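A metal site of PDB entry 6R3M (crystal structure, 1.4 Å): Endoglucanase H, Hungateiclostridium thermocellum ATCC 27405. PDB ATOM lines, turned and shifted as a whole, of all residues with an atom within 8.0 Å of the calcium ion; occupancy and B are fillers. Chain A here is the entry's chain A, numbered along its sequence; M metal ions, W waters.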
ATOM      1  N   MET A   9      14.349  19.656  19.585  1.00  0.00           N
ATOM      2  CA  MET A   9      14.782  19.681  18.181  1.00  0.00           C
ATOM      3  C   MET A   9      14.743  21.090  17.639  1.00  0.00           C
ATOM      4  O   MET A   9      13.739  21.785  17.781  1.00  0.00           O
ATOM      5  CB  MET A   9      13.925  18.749  17.312  1.00  0.00           C
ATOM      6  CG  MET A   9      14.421  18.569  15.845  1.00  0.00           C
ATOM      7  SD  MET A   9      16.019  17.748  15.760  1.00  0.00           S
ATOM      8  CE  MET A   9      15.579  16.116  16.366  1.00  0.00           C
ATOM      9  N   ASP A  11      16.300  21.621  14.240  1.00  0.00           N
ATOM     10  CA  ASP A  11      16.089  21.341  12.812  1.00  0.00           C
ATOM     11  C   ASP A  11      16.394  19.893  12.517  1.00  0.00           C
ATOM     12  O   ASP A  11      17.545  19.465  12.601  1.00  0.00           O
ATOM     13  CB  ASP A  11      16.874  22.281  11.879  1.00  0.00           C
ATOM     14  CG  ASP A  11      16.248  22.418  10.506  1.00  0.00           C
ATOM     15  OD1 ASP A  11      15.405  21.519  10.148  1.00  0.00           O
ATOM     16  OD2 ASP A  11      16.600  23.371   9.811  1.00  0.00           O
ATOM     17  N   ASP A  12      15.364  19.122  12.180  1.00  0.00           N
ATOM     18  CA  ASP A  12      15.560  17.751  11.748  1.00  0.00           C
ATOM     19  C   ASP A  12      15.537  17.698  10.214  1.00  0.00           C
ATOM     20  O   ASP A  12      15.617  16.609   9.658  1.00  0.00           O
ATOM     21  CB  ASP A  12      14.504  16.831  12.364  1.00  0.00           C
ATOM     22  CG  ASP A  12      13.066  17.170  11.975  1.00  0.00           C
ATOM     23  OD1 ASP A  12      12.834  18.059  11.083  1.00  0.00           O
ATOM     24  OD2 ASP A  12      12.146  16.565  12.622  1.00  0.00           O
ATOM     25  N   PHE A  13      15.426  18.856   9.540  1.00  0.00           N
ATOM     26  CA  PHE A  13      15.493  18.942   8.071  1.00  0.00           C
ATOM     27  C   PHE A  13      14.317  18.276   7.353  1.00  0.00           C
ATOM     28  O   PHE A  13      14.393  18.080   6.140  1.00  0.00           O
ATOM     29  CB  PHE A  13      16.858  18.505   7.511  1.00  0.00           C
ATOM     30  CG  PHE A  13      17.939  19.420   8.068  1.00  0.00           C
ATOM     31  CD1 PHE A  13      18.136  20.666   7.495  1.00  0.00           C
ATOM     32  CD2 PHE A  13      18.639  19.063   9.209  1.00  0.00           C
ATOM     33  CE1 PHE A  13      19.068  21.561   8.022  1.00  0.00           C
ATOM     34  CE2 PHE A  13      19.531  19.972   9.784  1.00  0.00           C
ATOM     35  CZ  PHE A  13      19.766  21.200   9.173  1.00  0.00           C
ATOM     36  N   GLU A  14      13.248  17.970   8.104  1.00  0.00           N
ATOM     37  CA  GLU A  14      12.094  17.317   7.475  1.00  0.00           C
ATOM     38  C   GLU A  14      11.025  18.345   7.118  1.00  0.00           C
ATOM     39  O   GLU A  14       9.966  17.981   6.553  1.00  0.00           O
ATOM     40  CB  GLU A  14      11.470  16.326   8.471  1.00  0.00           C
ATOM     41  CG  GLU A  14      12.387  15.302   9.080  1.00  0.00           C
ATOM     42  CD  GLU A  14      13.246  14.516   8.104  1.00  0.00           C
ATOM     43  OE1 GLU A  14      12.839  14.387   6.946  1.00  0.00           O
ATOM     44  OE2 GLU A  14      14.303  14.034   8.472  1.00  0.00           O
ATOM     45  N   GLY A  15      11.213  19.619   7.467  1.00  0.00           N
ATOM     46  CA  GLY A  15      10.197  20.668   7.255  1.00  0.00           C
ATOM     47  C   GLY A  15      10.680  21.901   6.478  1.00  0.00           C
ATOM     48  O   GLY A  15      11.197  21.799   5.374  1.00  0.00           O
ATOM     49  N   VAL A  34      18.967  16.781   1.009  1.00  0.00           N
ATOM     50  CA  VAL A  34      19.381  15.457   0.548  1.00  0.00           C
ATOM     51  C   VAL A  34      18.967  14.432   1.595  1.00  0.00           C
ATOM     52  O   VAL A  34      18.475  14.811   2.660  1.00  0.00           O
ATOM     53  CB  VAL A  34      20.895  15.376   0.279  1.00  0.00           C
ATOM     54  CG1 VAL A  34      21.330  16.383  -0.802  1.00  0.00           C
ATOM     55  CG2 VAL A  34      21.706  15.620   1.555  1.00  0.00           C
ATOM     56  N   SER A  35      19.188  13.136   1.306  1.00  0.00           N
ATOM     57  CA  SER A  35      19.093  12.111   2.339  1.00  0.00           C
ATOM     58  C   SER A  35      20.010  12.428   3.528  1.00  0.00           C
ATOM     59  O   SER A  35      21.155  12.837   3.398  1.00  0.00           O
ATOM     60  CB  SER A  35      19.364  10.750   1.789  1.00  0.00           C
ATOM     61  OG  SER A  35      18.261  10.450   0.968  1.00  0.00           O
ATOM     62  N   GLY A  36      19.446  12.228   4.721  1.00  0.00           N
ATOM     63  CA  GLY A  36      20.132  12.607   5.951  1.00  0.00           C
ATOM     64  C   GLY A  36      20.516  11.381   6.760  1.00  0.00           C
ATOM     65  O   GLY A  36      20.768  10.281   6.218  1.00  0.00           O
ATOM     66  N   LYS A  37      20.572  11.562   8.084  1.00  0.00           N
ATOM     67  CA  LYS A  37      20.922  10.483   8.989  1.00  0.00           C
ATOM     68  C   LYS A  37      19.639   9.679   9.226  1.00  0.00           C
ATOM     69  O   LYS A  37      19.634   8.453   9.081  1.00  0.00           O
ATOM     70  CB  LYS A  37      21.512  11.051  10.290  1.00  0.00           C
ATOM     71  CG  LYS A  37      22.122  10.009  11.231  1.00  0.00           C
ATOM     72  CD  LYS A  37      21.251   9.664  12.401  1.00  0.00           C
ATOM     73  CE  LYS A  37      22.075   8.970  13.462  1.00  0.00           C
ATOM     74  NZ  LYS A  37      21.204   8.295  14.462  1.00  0.00           N
ATOM     75  N   THR A  38      18.564  10.400   9.575  1.00  0.00           N
ATOM     76  CA  THR A  38      17.211   9.878   9.538  1.00  0.00           C
ATOM     77  C   THR A  38      16.386  10.808   8.659  1.00  0.00           C
ATOM     78  O   THR A  38      16.467  12.049   8.776  1.00  0.00           O
ATOM     79  CB  THR A  38      16.596   9.736  10.933  1.00  0.00           C
ATOM     80  OG1 THR A  38      16.726  10.980  11.640  1.00  0.00           O
ATOM     81  CG2 THR A  38      17.275   8.635  11.720  1.00  0.00           C
ATOM     82  N   GLY A  39      15.616  10.267   7.677  1.00  0.00           N
ATOM     83  CA  GLY A  39      14.898  11.157   6.794  1.00  0.00           C
ATOM     84  C   GLY A  39      15.871  11.987   5.934  1.00  0.00           C
ATOM     85  O   GLY A  39      16.854  11.457   5.381  1.00  0.00           O
ATOM     86  N   ASN A  40      15.556  13.266   5.803  1.00  0.00           N
ATOM     87  CA  ASN A  40      16.387  14.190   5.032  1.00  0.00           C
ATOM     88  C   ASN A  40      17.362  14.941   5.951  1.00  0.00           C
ATOM     89  O   ASN A  40      17.172  14.983   7.186  1.00  0.00           O
ATOM     90  CB  ASN A  40      15.535  15.192   4.269  1.00  0.00           C
ATOM     91  CG  ASN A  40      14.878  14.530   3.070  1.00  0.00           C
ATOM     92  OD1 ASN A  40      15.402  13.542   2.583  1.00  0.00           O
ATOM     93  ND2 ASN A  40      13.774  15.087   2.604  1.00  0.00           N
ATOM     94  N   GLY A  41      18.349  15.565   5.309  1.00  0.00           N
ATOM     95  CA  GLY A  41      19.397  16.352   5.932  1.00  0.00           C
ATOM     96  C   GLY A  41      19.729  17.484   4.974  1.00  0.00           C
ATOM     97  O   GLY A  41      19.143  17.591   3.889  1.00  0.00           O
ATOM     98  N   MET A  42      20.664  18.327   5.373  1.00  0.00           N
ATOM     99  CA  MET A  42      21.096  19.417   4.519  1.00  0.00           C
ATOM    100  C   MET A  42      22.552  19.217   4.126  1.00  0.00           C
ATOM    101  O   MET A  42      23.434  19.044   4.968  1.00  0.00           O
ATOM    102  CB  MET A  42      20.989  20.758   5.255  1.00  0.00           C
ATOM    103  CG  MET A  42      21.605  21.911   4.434  1.00  0.00           C
ATOM    104  SD  MET A  42      21.364  23.544   5.209  1.00  0.00           S
ATOM    105  CE  MET A  42      22.356  23.382   6.694  1.00  0.00           C
ATOM    106  N   ASP A  74      24.188  15.863  13.923  1.00  0.00           N
ATOM    107  CA  ASP A  74      24.816  14.758  13.228  1.00  0.00           C
ATOM    108  C   ASP A  74      25.512  15.341  12.000  1.00  0.00           C
ATOM    109  O   ASP A  74      24.964  16.225  11.342  1.00  0.00           O
ATOM    110  CB  ASP A  74      23.805  13.707  12.788  1.00  0.00           C
ATOM    111  CG  ASP A  74      22.998  13.166  13.953  1.00  0.00           C
ATOM    112  OD1 ASP A  74      23.476  13.226  15.087  1.00  0.00           O
ATOM    113  OD2 ASP A  74      21.846  12.771  13.712  1.00  0.00           O
ATOM    114  N   TRP A 113      28.542   8.895   9.613  1.00  0.00           N
ATOM    115  CA  TRP A 113      27.713   9.743  10.477  1.00  0.00           C
ATOM    116  C   TRP A 113      28.267   9.738  11.885  1.00  0.00           C
ATOM    117  O   TRP A 113      28.547   8.681  12.469  1.00  0.00           O
ATOM    118  CB  TRP A 113      26.256   9.297  10.512  1.00  0.00           C
ATOM    119  CG  TRP A 113      25.481   9.675   9.300  1.00  0.00           C
ATOM    120  CD1 TRP A 113      25.123   8.876   8.241  1.00  0.00           C
ATOM    121  CD2 TRP A 113      25.032  11.015   8.975  1.00  0.00           C
ATOM    122  NE1 TRP A 113      24.433   9.622   7.316  1.00  0.00           N
ATOM    123  CE2 TRP A 113      24.349  10.932   7.739  1.00  0.00           C
ATOM    124  CE3 TRP A 113      25.140  12.246   9.615  1.00  0.00           C
ATOM    125  CZ2 TRP A 113      23.800  12.064   7.123  1.00  0.00           C
ATOM    126  CZ3 TRP A 113      24.569  13.357   9.018  1.00  0.00           C
ATOM    127  CH2 TRP A 113      23.925  13.269   7.771  1.00  0.00           C
ATOM    128  N   VAL A 162      24.447  17.604   7.277  1.00  0.00           N
ATOM    129  CA  VAL A 162      24.072  17.683   8.679  1.00  0.00           C
ATOM    130  C   VAL A 162      22.625  17.243   8.884  1.00  0.00           C
ATOM    131  O   VAL A 162      21.778  17.305   7.992  1.00  0.00           O
ATOM    132  CB  VAL A 162      24.306  19.112   9.217  1.00  0.00           C
ATOM    133  CG1 VAL A 162      25.784  19.512   9.161  1.00  0.00           C
ATOM    134  CG2 VAL A 162      23.457  20.166   8.495  1.00  0.00           C
ATOM    135  N   ASP A 163      22.332  16.838  10.119  1.00  0.00           N
ATOM    136  CA  ASP A 163      20.986  16.446  10.470  1.00  0.00           C
ATOM    137  C   ASP A 163      20.820  16.645  11.977  1.00  0.00           C
ATOM    138  O   ASP A 163      21.788  16.795  12.705  1.00  0.00           O
ATOM    139  CB  ASP A 163      20.710  14.983  10.051  1.00  0.00           C
ATOM    140  CG  ASP A 163      19.238  14.651   9.857  1.00  0.00           C
ATOM    141  OD1 ASP A 163      18.335  15.485  10.166  1.00  0.00           O
ATOM    142  OD2 ASP A 163      18.990  13.472   9.359  1.00  0.00           O
ATOM    143  N   ASN A 164      19.546  16.679  12.411  1.00  0.00           N
ATOM    144  CA  ASN A 164      19.172  16.546  13.816  1.00  0.00           C
ATOM    145  C   ASN A 164      19.878  17.557  14.712  1.00  0.00           C
ATOM    146  O   ASN A 164      20.501  17.185  15.716  1.00  0.00           O
ATOM    147  CB  ASN A 164      19.418  15.122  14.316  1.00  0.00           C
ATOM    148  CG  ASN A 164      18.511  14.134  13.588  1.00  0.00           C
ATOM    149  OD1 ASN A 164      17.337  14.406  13.398  1.00  0.00           O
ATOM    150  ND2 ASN A 164      19.095  13.037  13.125  1.00  0.00           N
ATOM    151  N   ILE A 165      19.772  18.827  14.333  1.00  0.00           N
ATOM    152  CA  ILE A 165      20.321  19.892  15.179  1.00  0.00           C
ATOM    153  C   ILE A 165      19.363  20.068  16.352  1.00  0.00           C
ATOM    154  O   ILE A 165      18.178  20.386  16.142  1.00  0.00           O
ATOM    155  CB  ILE A 165      20.557  21.177  14.390  1.00  0.00           C
ATOM    156  CG1 ILE A 165      21.433  20.827  13.164  1.00  0.00           C
ATOM    157  CG2 ILE A 165      21.234  22.214  15.297  1.00  0.00           C
ATOM    158  CD1 ILE A 165      21.503  21.912  12.112  1.00  0.00           C
HETATM  159 CA    CA M   1      16.425  14.361   9.233  1.00  0.00          CA
HETATM  160  O   HOH W   1      15.799  13.634  11.411  1.00  0.00           O
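Water W1 lies within hydrogen-bond range of the side-chain amide oxygen of Asn 164 and the side-chain hydroxyl of Thr 38.
OG1 of Thr 38 is in hydrogen-bond range of ND2 of Asn 164, 3.5 Å away.
The backbone carbonyl oxygen (O) of Asp 163 is in hydrogen-bond range of the backbone NH (N) of Asp 74 (2.8 Å).
The side-chain carboxylate (OD2) of Asp 163 lies close to the backbone NH (N) of Lys 37 (2.8 Å).
The side-chain amide oxygen (OD1) of Asn 40 sits close to the backbone carbonyl oxygen (O) of Val 34 (3.3 Å).
Of the 21 residues printed, 5 come within 4 Å of the calcium ion.
The nearest printed residue that does not touch the calcium ion is Gly 39 (4.1 Å).
The calcium ion is bound by O of Asn 40 (2.3 Å), OE2 of Glu 14 (2.3 Å), O of Thr 38 (2.4 Å), water W1 (2.4 Å), OD1 of Asp 163 (2.4 Å), O of Asp 12 (2.4 Å) and OD2 of Asp 163 (2.7 Å).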
